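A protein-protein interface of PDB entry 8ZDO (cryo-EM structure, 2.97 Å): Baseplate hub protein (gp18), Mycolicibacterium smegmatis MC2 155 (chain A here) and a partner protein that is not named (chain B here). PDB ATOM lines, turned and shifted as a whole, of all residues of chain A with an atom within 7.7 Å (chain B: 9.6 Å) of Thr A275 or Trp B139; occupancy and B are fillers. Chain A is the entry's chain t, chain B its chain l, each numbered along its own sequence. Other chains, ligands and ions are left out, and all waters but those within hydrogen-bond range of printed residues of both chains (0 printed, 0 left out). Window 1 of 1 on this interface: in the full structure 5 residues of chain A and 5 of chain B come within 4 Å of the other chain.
The backbone carbonyl oxygen (O) of Gly A273 lies within hydrogen-bond range of the backbone NH (N) of Trp B139 (3.3 Å). The side-chain hydroxyl of Thr A275 is in hydrogen-bond range of the backbone carbonyl oxygen of Trp B139.
The guanidinium group (NH2) of Arg A122 lies within salt-bridge range of the side-chain carboxylate (OE2) of Glu A274 (2.4 Å). O of Leu A269 lies close to N of Glu A274 (3.5 Å). The side-chain hydroxyl of Ser B141 is in hydrogen-bond range of the backbone carbonyl oxygen of Gly B138 (2.9 Å). The guanidinium group of Arg A266 lies within salt-bridge range of the side-chain carboxylate of Glu A274.
Among the printed residues, merely in contact across the chains: Gly A273 with Gly B138 (3.1 Å), Glu A274 with Trp B139 (3.7 Å) and Thr A275 with Asn B137 (3.5 Å).
Thr A275 touches just these residues of chain B: Asn B137 and Trp B139. Trp B139 touches just these residues of chain A: Gly A273, Glu A274 and Thr A275. Ala A276 touches none of the printed residues of chain B. Printed residues of chain A within 4 Å of Asn B137: Thr A275. Of the printed residues of chain A, Gly B138 touches Gly A273. The nearest residue of chain A that does not touch Trp B139 is Arg A266 (4.1 Å).
Printed residues of chain B that touch a printed residue of chain A: Asn B137, Gly B138 and Trp B139. Hydrophobic or aromatic side chains of chain B that line the printed part of chain A: Trp B139. Of the 20 printed residues of chain A, 3 touch a printed residue of chain B. Among the printed residues, no Asp or Glu carboxylate lies within 4 Å of a Lys or Arg side-chain nitrogen of the other chain.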
ATOM      1  N   ASP A 115     -24.697 -26.613  -7.785  1.00  0.00           N
ATOM      2  CA  ASP A 115     -23.377 -26.007  -7.687  1.00  0.00           C
ATOM      3  C   ASP A 115     -22.715 -26.451  -6.392  1.00  0.00           C
ATOM      4  O   ASP A 115     -23.296 -26.304  -5.313  1.00  0.00           O
ATOM      5  CB  ASP A 115     -23.467 -24.484  -7.743  1.00  0.00           C
ATOM      6  CG  ASP A 115     -23.518 -23.957  -9.159  1.00  0.00           C
ATOM      7  OD1 ASP A 115     -23.532 -24.779 -10.098  1.00  0.00           O
ATOM      8  OD2 ASP A 115     -23.546 -22.723  -9.336  1.00  0.00           O
ATOM      9  N   GLY A 118     -19.171 -23.152  -4.611  1.00  0.00           N
ATOM     10  CA  GLY A 118     -19.437 -21.867  -5.231  1.00  0.00           C
ATOM     11  C   GLY A 118     -19.477 -21.907  -6.742  1.00  0.00           C
ATOM     12  O   GLY A 118     -18.980 -20.981  -7.395  1.00  0.00           O
ATOM     13  N   GLY A 119     -20.052 -22.957  -7.315  1.00  0.00           N
ATOM     14  CA  GLY A 119     -20.162 -23.076  -8.751  1.00  0.00           C
ATOM     15  C   GLY A 119     -18.947 -23.635  -9.451  1.00  0.00           C
ATOM     16  O   GLY A 119     -18.974 -23.775 -10.680  1.00  0.00           O
ATOM     17  N   LYS A 120     -17.877 -23.951  -8.718  1.00  0.00           N
ATOM     18  CA  LYS A 120     -16.703 -24.548  -9.348  1.00  0.00           C
ATOM     19  C   LYS A 120     -17.029 -25.916  -9.929  1.00  0.00           C
ATOM     20  O   LYS A 120     -16.578 -26.254 -11.029  1.00  0.00           O
ATOM     21  CB  LYS A 120     -15.560 -24.647  -8.341  1.00  0.00           C
ATOM     22  CG  LYS A 120     -14.842 -23.333  -8.088  1.00  0.00           C
ATOM     23  CD  LYS A 120     -13.810 -23.485  -6.986  1.00  0.00           C
ATOM     24  CE  LYS A 120     -13.158 -22.160  -6.643  1.00  0.00           C
ATOM     25  NZ  LYS A 120     -12.324 -22.267  -5.416  1.00  0.00           N
ATOM     26  N   ARG A 122     -20.259 -28.150 -11.203  1.00  0.00           N
ATOM     27  CA  ARG A 122     -21.665 -27.959 -11.533  1.00  0.00           C
ATOM     28  C   ARG A 122     -22.231 -29.196 -12.205  1.00  0.00           C
ATOM     29  O   ARG A 122     -21.629 -29.738 -13.135  1.00  0.00           O
ATOM     30  CB  ARG A 122     -21.869 -26.737 -12.434  1.00  0.00           C
ATOM     31  CG  ARG A 122     -23.322 -26.512 -12.812  1.00  0.00           C
ATOM     32  CD  ARG A 122     -23.512 -25.235 -13.596  1.00  0.00           C
ATOM     33  NE  ARG A 122     -23.359 -24.059 -12.751  1.00  0.00           N
ATOM     34  CZ  ARG A 122     -23.022 -22.858 -13.197  1.00  0.00           C
ATOM     35  NH1 ARG A 122     -22.806 -22.634 -14.482  1.00  0.00           N
ATOM     36  NH2 ARG A 122     -22.898 -21.856 -12.332  1.00  0.00           N
ATOM     37  N   ARG A 266     -20.251 -27.448 -19.712  1.00  0.00           N
ATOM     38  CA  ARG A 266     -20.522 -26.404 -18.735  1.00  0.00           C
ATOM     39  C   ARG A 266     -21.675 -25.554 -19.234  1.00  0.00           C
ATOM     40  O   ARG A 266     -21.659 -25.099 -20.380  1.00  0.00           O
ATOM     41  CB  ARG A 266     -19.288 -25.533 -18.489  1.00  0.00           C
ATOM     42  CG  ARG A 266     -19.521 -24.416 -17.492  1.00  0.00           C
ATOM     43  CD  ARG A 266     -18.982 -24.782 -16.127  1.00  0.00           C
ATOM     44  NE  ARG A 266     -19.201 -23.717 -15.157  1.00  0.00           N
ATOM     45  CZ  ARG A 266     -19.201 -23.890 -13.843  1.00  0.00           C
ATOM     46  NH1 ARG A 266     -18.989 -25.079 -13.304  1.00  0.00           N
ATOM     47  NH2 ARG A 266     -19.421 -22.846 -13.051  1.00  0.00           N
ATOM     48  N   VAL A 268     -23.288 -22.162 -19.115  1.00  0.00           N
ATOM     49  CA  VAL A 268     -22.839 -20.819 -18.758  1.00  0.00           C
ATOM     50  C   VAL A 268     -24.039 -20.013 -18.279  1.00  0.00           C
ATOM     51  O   VAL A 268     -24.870 -19.579 -19.078  1.00  0.00           O
ATOM     52  CB  VAL A 268     -22.146 -20.128 -19.935  1.00  0.00           C
ATOM     53  CG1 VAL A 268     -21.582 -18.795 -19.500  1.00  0.00           C
ATOM     54  CG2 VAL A 268     -21.051 -21.015 -20.494  1.00  0.00           C
ATOM     55  N   LEU A 269     -24.123 -19.798 -16.969  1.00  0.00           N
ATOM     56  CA  LEU A 269     -25.175 -18.973 -16.382  1.00  0.00           C
ATOM     57  C   LEU A 269     -24.672 -17.538 -16.356  1.00  0.00           C
ATOM     58  O   LEU A 269     -24.008 -17.104 -15.415  1.00  0.00           O
ATOM     59  CB  LEU A 269     -25.539 -19.471 -14.989  1.00  0.00           C
ATOM     60  CG  LEU A 269     -26.234 -20.830 -14.911  1.00  0.00           C
ATOM     61  CD1 LEU A 269     -26.523 -21.185 -13.469  1.00  0.00           C
ATOM     62  CD2 LEU A 269     -27.508 -20.828 -15.731  1.00  0.00           C
ATOM     63  N   THR A 270     -24.991 -16.788 -17.412  1.00  0.00           N
ATOM     64  CA  THR A 270     -24.590 -15.388 -17.473  1.00  0.00           C
ATOM     65  C   THR A 270     -25.329 -14.532 -16.457  1.00  0.00           C
ATOM     66  O   THR A 270     -24.907 -13.402 -16.193  1.00  0.00           O
ATOM     67  CB  THR A 270     -24.808 -14.833 -18.879  1.00  0.00           C
ATOM     68  OG1 THR A 270     -26.182 -14.467 -19.041  1.00  0.00           O
ATOM     69  CG2 THR A 270     -24.435 -15.868 -19.922  1.00  0.00           C
ATOM     70  N   ASP A 272     -25.260 -15.269 -13.413  1.00  0.00           N
ATOM     71  CA  ASP A 272     -24.317 -15.312 -12.305  1.00  0.00           C
ATOM     72  C   ASP A 272     -23.039 -14.538 -12.593  1.00  0.00           C
ATOM     73  O   ASP A 272     -22.125 -14.547 -11.763  1.00  0.00           O
ATOM     74  CB  ASP A 272     -23.971 -16.764 -11.965  1.00  0.00           C
ATOM     75  CG  ASP A 272     -25.001 -17.415 -11.070  1.00  0.00           C
ATOM     76  OD1 ASP A 272     -26.194 -17.057 -11.178  1.00  0.00           O
ATOM     77  OD2 ASP A 272     -24.621 -18.282 -10.258  1.00  0.00           O
ATOM     78  N   GLY A 273     -22.953 -13.877 -13.743  1.00  0.00           N
ATOM     79  CA  GLY A 273     -21.751 -13.187 -14.144  1.00  0.00           C
ATOM     80  C   GLY A 273     -20.765 -14.021 -14.929  1.00  0.00           C
ATOM     81  O   GLY A 273     -19.753 -13.480 -15.388  1.00  0.00           O
ATOM     82  N   GLU A 274     -21.021 -15.314 -15.099  1.00  0.00           N
ATOM     83  CA  GLU A 274     -20.094 -16.164 -15.828  1.00  0.00           C
ATOM     84  C   GLU A 274     -20.078 -15.803 -17.307  1.00  0.00           C
ATOM     85  O   GLU A 274     -21.104 -15.442 -17.889  1.00  0.00           O
ATOM     86  CB  GLU A 274     -20.470 -17.633 -15.659  1.00  0.00           C
ATOM     87  CG  GLU A 274     -20.935 -17.998 -14.270  1.00  0.00           C
ATOM     88  CD  GLU A 274     -21.426 -19.423 -14.190  1.00  0.00           C
ATOM     89  OE1 GLU A 274     -21.074 -20.222 -15.084  1.00  0.00           O
ATOM     90  OE2 GLU A 274     -22.170 -19.746 -13.240  1.00  0.00           O
ATOM     91  N   THR A 275     -18.899 -15.901 -17.911  1.00  0.00           N
ATOM     92  CA  THR A 275     -18.713 -15.655 -19.330  1.00  0.00           C
ATOM     93  C   THR A 275     -18.014 -16.856 -19.950  1.00  0.00           C
ATOM     94  O   THR A 275     -17.584 -17.781 -19.256  1.00  0.00           O
ATOM     95  CB  THR A 275     -17.900 -14.377 -19.583  1.00  0.00           C
ATOM     96  OG1 THR A 275     -16.595 -14.517 -19.010  1.00  0.00           O
ATOM     97  CG2 THR A 275     -18.588 -13.172 -18.967  1.00  0.00           C
ATOM     98  N   ALA A 276     -17.905 -16.838 -21.274  1.00  0.00           N
ATOM     99  CA  ALA A 276     -17.232 -17.900 -22.002  1.00  0.00           C
ATOM    100  C   ALA A 276     -16.430 -17.295 -23.144  1.00  0.00           C
ATOM    101  O   ALA A 276     -16.713 -16.191 -23.613  1.00  0.00           O
ATOM    102  CB  ALA A 276     -18.227 -18.937 -22.536  1.00  0.00           C
ATOM    103  N   GLU A 277     -15.415 -18.033 -23.583  1.00  0.00           N
ATOM    104  CA  GLU A 277     -14.557 -17.581 -24.666  1.00  0.00           C
ATOM    105  C   GLU A 277     -13.930 -18.794 -25.331  1.00  0.00           C
ATOM    106  O   GLU A 277     -13.919 -19.894 -24.774  1.00  0.00           O
ATOM    107  CB  GLU A 277     -13.479 -16.618 -24.160  1.00  0.00           C
ATOM    108  CG  GLU A 277     -12.669 -17.149 -22.989  1.00  0.00           C
ATOM    109  CD  GLU A 277     -11.407 -17.865 -23.422  1.00  0.00           C
ATOM    110  OE1 GLU A 277     -10.913 -17.587 -24.535  1.00  0.00           O
ATOM    111  OE2 GLU A 277     -10.910 -18.710 -22.649  1.00  0.00           O
ATOM    112  N   PHE A 279     -14.716 -19.903 -28.610  1.00  0.00           N
ATOM    113  CA  PHE A 279     -15.523 -20.483 -29.670  1.00  0.00           C
ATOM    114  C   PHE A 279     -16.244 -19.362 -30.396  1.00  0.00           C
ATOM    115  O   PHE A 279     -16.371 -18.254 -29.866  1.00  0.00           O
ATOM    116  CB  PHE A 279     -16.527 -21.516 -29.134  1.00  0.00           C
ATOM    117  CG  PHE A 279     -17.305 -21.063 -27.932  1.00  0.00           C
ATOM    118  CD1 PHE A 279     -16.742 -21.089 -26.670  1.00  0.00           C
ATOM    119  CD2 PHE A 279     -18.614 -20.645 -28.063  1.00  0.00           C
ATOM    120  CE1 PHE A 279     -17.460 -20.687 -25.573  1.00  0.00           C
ATOM    121  CE2 PHE A 279     -19.337 -20.245 -26.966  1.00  0.00           C
ATOM    122  CZ  PHE A 279     -18.761 -20.267 -25.721  1.00  0.00           C
ATOM    123  N   ALA A 282     -18.823 -16.571 -28.773  1.00  0.00           N
ATOM    124  CA  ALA A 282     -18.728 -16.816 -27.340  1.00  0.00           C
ATOM    125  C   ALA A 282     -19.103 -15.608 -26.497  1.00  0.00           C
ATOM    126  O   ALA A 282     -19.318 -15.764 -25.291  1.00  0.00           O
ATOM    127  CB  ALA A 282     -17.317 -17.264 -26.980  1.00  0.00           C
ATOM    128  N   HIS A 283     -19.179 -14.417 -27.088  1.00  0.00           N
ATOM    129  CA  HIS A 283     -19.471 -13.214 -26.321  1.00  0.00           C
ATOM    130  C   HIS A 283     -20.960 -12.931 -26.204  1.00  0.00           C
ATOM    131  O   HIS A 283     -21.383 -12.280 -25.242  1.00  0.00           O
ATOM    132  CB  HIS A 283     -18.770 -12.009 -26.949  1.00  0.00           C
ATOM    133  CG  HIS A 283     -19.126 -11.784 -28.385  1.00  0.00           C
ATOM    134  ND1 HIS A 283     -20.281 -11.142 -28.775  1.00  0.00           N
ATOM    135  CD2 HIS A 283     -18.477 -12.115 -29.527  1.00  0.00           C
ATOM    136  CE1 HIS A 283     -20.330 -11.088 -30.094  1.00  0.00           C
ATOM    137  NE2 HIS A 283     -19.247 -11.672 -30.574  1.00  0.00           N
ATOM    138  N   ILE A 285     -23.454 -15.269 -26.037  1.00  0.00           N
ATOM    139  CA  ILE A 285     -24.220 -16.434 -25.615  1.00  0.00           C
ATOM    140  C   ILE A 285     -25.211 -16.037 -24.529  1.00  0.00           C
ATOM    141  O   ILE A 285     -24.980 -15.106 -23.746  1.00  0.00           O
ATOM    142  CB  ILE A 285     -23.294 -17.568 -25.139  1.00  0.00           C
ATOM    143  CG1 ILE A 285     -22.706 -17.250 -23.768  1.00  0.00           C
ATOM    144  CG2 ILE A 285     -22.185 -17.809 -26.140  1.00  0.00           C
ATOM    145  CD1 ILE A 285     -22.046 -18.432 -23.124  1.00  0.00           C
ATOM    146  N   VAL A 291     -21.868 -25.491 -23.221  1.00  0.00           N
ATOM    147  CA  VAL A 291     -20.617 -25.459 -23.970  1.00  0.00           C
ATOM    148  C   VAL A 291     -19.878 -26.767 -23.732  1.00  0.00           C
ATOM    149  O   VAL A 291     -19.713 -27.190 -22.583  1.00  0.00           O
ATOM    150  CB  VAL A 291     -19.731 -24.263 -23.572  1.00  0.00           C
ATOM    151  CG1 VAL A 291     -18.583 -24.118 -24.547  1.00  0.00           C
ATOM    152  CG2 VAL A 291     -20.540 -22.986 -23.524  1.00  0.00           C
ATOM    153  N   ILE B 128      -3.780 -13.854 -11.337  1.00  0.00           N
ATOM    154  CA  ILE B 128      -4.735 -12.976 -10.669  1.00  0.00           C
ATOM    155  C   ILE B 128      -4.829 -13.311  -9.187  1.00  0.00           C
ATOM    156  O   ILE B 128      -4.774 -12.425  -8.327  1.00  0.00           O
ATOM    157  CB  ILE B 128      -6.109 -13.060 -11.354  1.00  0.00           C
ATOM    158  CG1 ILE B 128      -6.043 -12.442 -12.750  1.00  0.00           C
ATOM    159  CG2 ILE B 128      -7.165 -12.364 -10.517  1.00  0.00           C
ATOM    160  CD1 ILE B 128      -5.656 -10.990 -12.743  1.00  0.00           C
ATOM    161  N   TRP B 132      -9.189 -11.600  -5.788  1.00  0.00           N
ATOM    162  CA  TRP B 132      -9.788 -10.563  -6.619  1.00  0.00           C
ATOM    163  C   TRP B 132     -10.983 -11.152  -7.352  1.00  0.00           C
ATOM    164  O   TRP B 132     -10.843 -12.145  -8.074  1.00  0.00           O
ATOM    165  CB  TRP B 132      -8.771 -10.006  -7.613  1.00  0.00           C
ATOM    166  CG  TRP B 132      -7.683  -9.213  -6.975  1.00  0.00           C
ATOM    167  CD1 TRP B 132      -6.397  -9.607  -6.773  1.00  0.00           C
ATOM    168  CD2 TRP B 132      -7.782  -7.883  -6.455  1.00  0.00           C
ATOM    169  NE1 TRP B 132      -5.687  -8.608  -6.158  1.00  0.00           N
ATOM    170  CE2 TRP B 132      -6.516  -7.538  -5.953  1.00  0.00           C
ATOM    171  CE3 TRP B 132      -8.818  -6.952  -6.369  1.00  0.00           C
ATOM    172  CZ2 TRP B 132      -6.258  -6.301  -5.370  1.00  0.00           C
ATOM    173  CZ3 TRP B 132      -8.561  -5.727  -5.789  1.00  0.00           C
ATOM    174  CH2 TRP B 132      -7.293  -5.413  -5.297  1.00  0.00           C
ATOM    175  N   LYS B 133     -12.152 -10.539  -7.175  1.00  0.00           N
ATOM    176  CA  LYS B 133     -13.366 -10.998  -7.824  1.00  0.00           C
ATOM    177  C   LYS B 133     -13.679 -10.091  -8.998  1.00  0.00           C
ATOM    178  O   LYS B 133     -13.925  -8.894  -8.789  1.00  0.00           O
ATOM    179  CB  LYS B 133     -14.528 -11.008  -6.840  1.00  0.00           C
ATOM    180  CG  LYS B 133     -15.858 -11.363  -7.469  1.00  0.00           C
ATOM    181  CD  LYS B 133     -16.923 -11.603  -6.419  1.00  0.00           C
ATOM    182  CE  LYS B 133     -18.258 -11.022  -6.852  1.00  0.00           C
ATOM    183  NZ  LYS B 133     -19.261 -11.040  -5.753  1.00  0.00           N
ATOM    184  N   PRO B 134     -13.653 -10.589 -10.233  1.00  0.00           N
ATOM    185  CA  PRO B 134     -13.968  -9.729 -11.379  1.00  0.00           C
ATOM    186  C   PRO B 134     -15.399  -9.220 -11.309  1.00  0.00           C
ATOM    187  O   PRO B 134     -16.308  -9.927 -10.870  1.00  0.00           O
ATOM    188  CB  PRO B 134     -13.753 -10.650 -12.584  1.00  0.00           C
ATOM    189  CG  PRO B 134     -12.910 -11.770 -12.077  1.00  0.00           C
ATOM    190  CD  PRO B 134     -13.284 -11.951 -10.646  1.00  0.00           C
ATOM    191  N   MET B 135     -15.591  -7.980 -11.750  1.00  0.00           N
ATOM    192  CA  MET B 135     -16.888  -7.325 -11.718  1.00  0.00           C
ATOM    193  C   MET B 135     -17.054  -6.459 -12.957  1.00  0.00           C
ATOM    194  O   MET B 135     -16.078  -5.970 -13.542  1.00  0.00           O
ATOM    195  CB  MET B 135     -17.067  -6.458 -10.461  1.00  0.00           C
ATOM    196  CG  MET B 135     -16.884  -7.197  -9.147  1.00  0.00           C
ATOM    197  SD  MET B 135     -17.977  -6.609  -7.844  1.00  0.00           S
ATOM    198  CE  MET B 135     -19.388  -7.681  -8.084  1.00  0.00           C
ATOM    199  N   GLY B 136     -18.314  -6.259 -13.333  1.00  0.00           N
ATOM    200  CA  GLY B 136     -18.655  -5.485 -14.505  1.00  0.00           C
ATOM    201  C   GLY B 136     -18.718  -6.332 -15.756  1.00  0.00           C
ATOM    202  O   GLY B 136     -19.752  -6.389 -16.426  1.00  0.00           O
ATOM    203  N   ASN B 137     -17.613  -7.000 -16.079  1.00  0.00           N
ATOM    204  CA  ASN B 137     -17.519  -7.815 -17.280  1.00  0.00           C
ATOM    205  C   ASN B 137     -17.493  -9.306 -16.989  1.00  0.00           C
ATOM    206  O   ASN B 137     -17.342 -10.101 -17.922  1.00  0.00           O
ATOM    207  CB  ASN B 137     -16.277  -7.422 -18.083  1.00  0.00           C
ATOM    208  CG  ASN B 137     -16.396  -6.046 -18.689  1.00  0.00           C
ATOM    209  OD1 ASN B 137     -17.479  -5.469 -18.737  1.00  0.00           O
ATOM    210  ND2 ASN B 137     -15.281  -5.511 -19.159  1.00  0.00           N
ATOM    211  N   GLY B 138     -17.631  -9.708 -15.734  1.00  0.00           N
ATOM    212  CA  GLY B 138     -17.731 -11.112 -15.411  1.00  0.00           C
ATOM    213  C   GLY B 138     -16.390 -11.809 -15.310  1.00  0.00           C
ATOM    214  O   GLY B 138     -15.318 -11.200 -15.336  1.00  0.00           O
ATOM    215  N   TRP B 139     -16.471 -13.133 -15.196  1.00  0.00           N
ATOM    216  CA  TRP B 139     -15.290 -13.951 -14.954  1.00  0.00           C
ATOM    217  C   TRP B 139     -14.324 -13.873 -16.129  1.00  0.00           C
ATOM    218  O   TRP B 139     -14.734 -13.861 -17.293  1.00  0.00           O
ATOM    219  CB  TRP B 139     -15.696 -15.404 -14.716  1.00  0.00           C
ATOM    220  CG  TRP B 139     -16.559 -15.614 -13.510  1.00  0.00           C
ATOM    221  CD1 TRP B 139     -16.972 -14.667 -12.619  1.00  0.00           C
ATOM    222  CD2 TRP B 139     -17.119 -16.854 -13.066  1.00  0.00           C
ATOM    223  NE1 TRP B 139     -17.754 -15.241 -11.648  1.00  0.00           N
ATOM    224  CE2 TRP B 139     -17.860 -16.584 -11.898  1.00  0.00           C
ATOM    225  CE3 TRP B 139     -17.066 -18.167 -13.541  1.00  0.00           C
ATOM    226  CZ2 TRP B 139     -18.540 -17.577 -11.200  1.00  0.00           C
ATOM    227  CZ3 TRP B 139     -17.744 -19.153 -12.846  1.00  0.00           C
ATOM    228  CH2 TRP B 139     -18.471 -18.852 -11.688  1.00  0.00           C
ATOM    229  N   GLY B 140     -13.032 -13.826 -15.816  1.00  0.00           N
ATOM    230  CA  GLY B 140     -12.010 -13.786 -16.839  1.00  0.00           C
ATOM    231  C   GLY B 140     -11.766 -12.431 -17.459  1.00  0.00           C
ATOM    232  O   GLY B 140     -11.126 -12.360 -18.514  1.00  0.00           O
ATOM    233  N   SER B 141     -12.254 -11.356 -16.847  1.00  0.00           N
ATOM    234  CA  SER B 141     -12.054 -10.015 -17.378  1.00  0.00           C
ATOM    235  C   SER B 141     -10.755  -9.373 -16.913  1.00  0.00           C
ATOM    236  O   SER B 141     -10.394  -8.308 -17.422  1.00  0.00           O
ATOM    237  CB  SER B 141     -13.230  -9.116 -16.991  1.00  0.00           C
ATOM    238  OG  SER B 141     -13.381  -9.053 -15.585  1.00  0.00           O
ATOM    239  N   LEU B 142     -10.045  -9.986 -15.975  1.00  0.00           N
ATOM    240  CA  LEU B 142      -8.811  -9.438 -15.438  1.00  0.00           C
ATOM    241  C   LEU B 142      -7.602 -10.157 -16.017  1.00  0.00           C
ATOM    242  O   LEU B 142      -7.694 -11.280 -16.519  1.00  0.00           O
ATOM    243  CB  LEU B 142      -8.798  -9.538 -13.912  1.00  0.00           C
ATOM    244  CG  LEU B 142      -9.956  -8.850 -13.195  1.00  0.00           C
ATOM    245  CD1 LEU B 142     -10.108  -9.401 -11.792  1.00  0.00           C
ATOM    246  CD2 LEU B 142      -9.740  -7.353 -13.164  1.00  0.00           C
ATOM    247  N   GLY B 143      -6.454  -9.491 -15.937  1.00  0.00           N
ATOM    248  CA  GLY B 143      -5.221 -10.057 -16.450  1.00  0.00           C
ATOM    249  C   GLY B 143      -4.018  -9.366 -15.851  1.00  0.00           C
ATOM    250  O   GLY B 143      -4.124  -8.320 -15.206  1.00  0.00           O
ATOM    251  N   ASN B 159      -8.631  -7.715 -19.032  1.00  0.00           N
ATOM    252  CA  ASN B 159      -8.263  -8.700 -20.044  1.00  0.00           C
ATOM    253  C   ASN B 159      -8.450  -8.047 -21.405  1.00  0.00           C
ATOM    254  O   ASN B 159      -9.559  -8.006 -21.943  1.00  0.00           O
ATOM    255  CB  ASN B 159      -9.109  -9.959 -19.905  1.00  0.00           C
ATOM    256  CG  ASN B 159      -8.526 -11.132 -20.656  1.00  0.00           C
ATOM    257  OD1 ASN B 159      -7.431 -11.048 -21.209  1.00  0.00           O
ATOM    258  ND2 ASN B 159      -9.255 -12.241 -20.678  1.00  0.00           N
ATOM    259  N   LEU B 162     -10.247  -9.513 -24.499  1.00  0.00           N
ATOM    260  CA  LEU B 162     -11.702  -9.514 -24.564  1.00  0.00           C
ATOM    261  C   LEU B 162     -12.333  -8.161 -24.271  1.00  0.00           C
ATOM    262  O   LEU B 162     -13.291  -7.780 -24.946  1.00  0.00           O
ATOM    263  CB  LEU B 162     -12.271 -10.553 -23.589  1.00  0.00           C
ATOM    264  CG  LEU B 162     -11.553 -11.899 -23.512  1.00  0.00           C
ATOM    265  CD1 LEU B 162     -12.142 -12.749 -22.402  1.00  0.00           C
ATOM    266  CD2 LEU B 162     -11.632 -12.623 -24.845  1.00  0.00           C
ATOM    267  N   PHE B 163     -11.828  -7.423 -23.284  1.00  0.00           N
ATOM    268  CA  PHE B 163     -12.470  -6.199 -22.828  1.00  0.00           C
ATOM    269  C   PHE B 163     -11.473  -5.051 -22.786  1.00  0.00           C
ATOM    270  O   PHE B 163     -10.258  -5.249 -22.766  1.00  0.00           O
ATOM    271  CB  PHE B 163     -13.090  -6.364 -21.433  1.00  0.00           C
ATOM    272  CG  PHE B 163     -13.829  -7.651 -21.239  1.00  0.00           C
ATOM    273  CD1 PHE B 163     -15.155  -7.765 -21.614  1.00  0.00           C
ATOM    274  CD2 PHE B 163     -13.205  -8.743 -20.664  1.00  0.00           C
ATOM    275  CE1 PHE B 163     -15.841  -8.944 -21.431  1.00  0.00           C
ATOM    276  CE2 PHE B 163     -13.888  -9.927 -20.479  1.00  0.00           C
ATOM    277  CZ  PHE B 163     -15.207 -10.026 -20.863  1.00  0.00           C
ATOM    278  N   ALA B 166     -12.871  -3.009 -16.926  1.00  0.00           N
ATOM    279  CA  ALA B 166     -13.086  -4.092 -15.971  1.00  0.00           C
ATOM    280  C   ALA B 166     -13.103  -3.514 -14.564  1.00  0.00           C
ATOM    281  O   ALA B 166     -12.679  -2.378 -14.337  1.00  0.00           O
ATOM    282  CB  ALA B 166     -12.010  -5.173 -16.095  1.00  0.00           C
ATOM    283  N   ALA B 167     -13.581  -4.320 -13.613  1.00  0.00           N
ATOM    284  CA  ALA B 167     -13.465  -3.983 -12.205  1.00  0.00           C
ATOM    285  C   ALA B 167     -13.053  -5.229 -11.441  1.00  0.00           C
ATOM    286  O   ALA B 167     -13.261  -6.354 -11.892  1.00  0.00           O
ATOM    287  CB  ALA B 167     -14.775  -3.419 -11.646  1.00  0.00           C
ATOM    288  N   LEU B 171     -11.775  -9.673  -2.269  1.00  0.00           N
ATOM    289  CA  LEU B 171     -12.731 -10.699  -1.859  1.00  0.00           C
ATOM    290  C   LEU B 171     -13.329 -10.409  -0.489  1.00  0.00           C
ATOM    291  O   LEU B 171     -14.543 -10.534  -0.297  1.00  0.00           O
ATOM    292  CB  LEU B 171     -12.055 -12.067  -1.864  1.00  0.00           C
ATOM    293  CG  LEU B 171     -12.985 -13.258  -2.069  1.00  0.00           C
ATOM    294  CD1 LEU B 171     -13.688 -13.152  -3.405  1.00  0.00           C
ATOM    295  CD2 LEU B 171     -12.206 -14.551  -1.969  1.00  0.00           C
ATOM    296  N   GLN B 202     -21.928  -5.671  -4.523  1.00  0.00           N
ATOM    297  CA  GLN B 202     -21.876  -5.736  -5.976  1.00  0.00           C
ATOM    298  C   GLN B 202     -21.238  -4.503  -6.599  1.00  0.00           C
ATOM    299  O   GLN B 202     -21.326  -4.325  -7.817  1.00  0.00           O
ATOM    300  CB  GLN B 202     -23.282  -5.938  -6.543  1.00  0.00           C
ATOM    301  CG  GLN B 202     -23.992  -7.166  -6.012  1.00  0.00           C
ATOM    302  CD  GLN B 202     -23.543  -8.435  -6.701  1.00  0.00           C
ATOM    303  OE1 GLN B 202     -23.224  -8.430  -7.887  1.00  0.00           O
ATOM    304  NE2 GLN B 202     -23.520  -9.533  -5.959  1.00  0.00           N
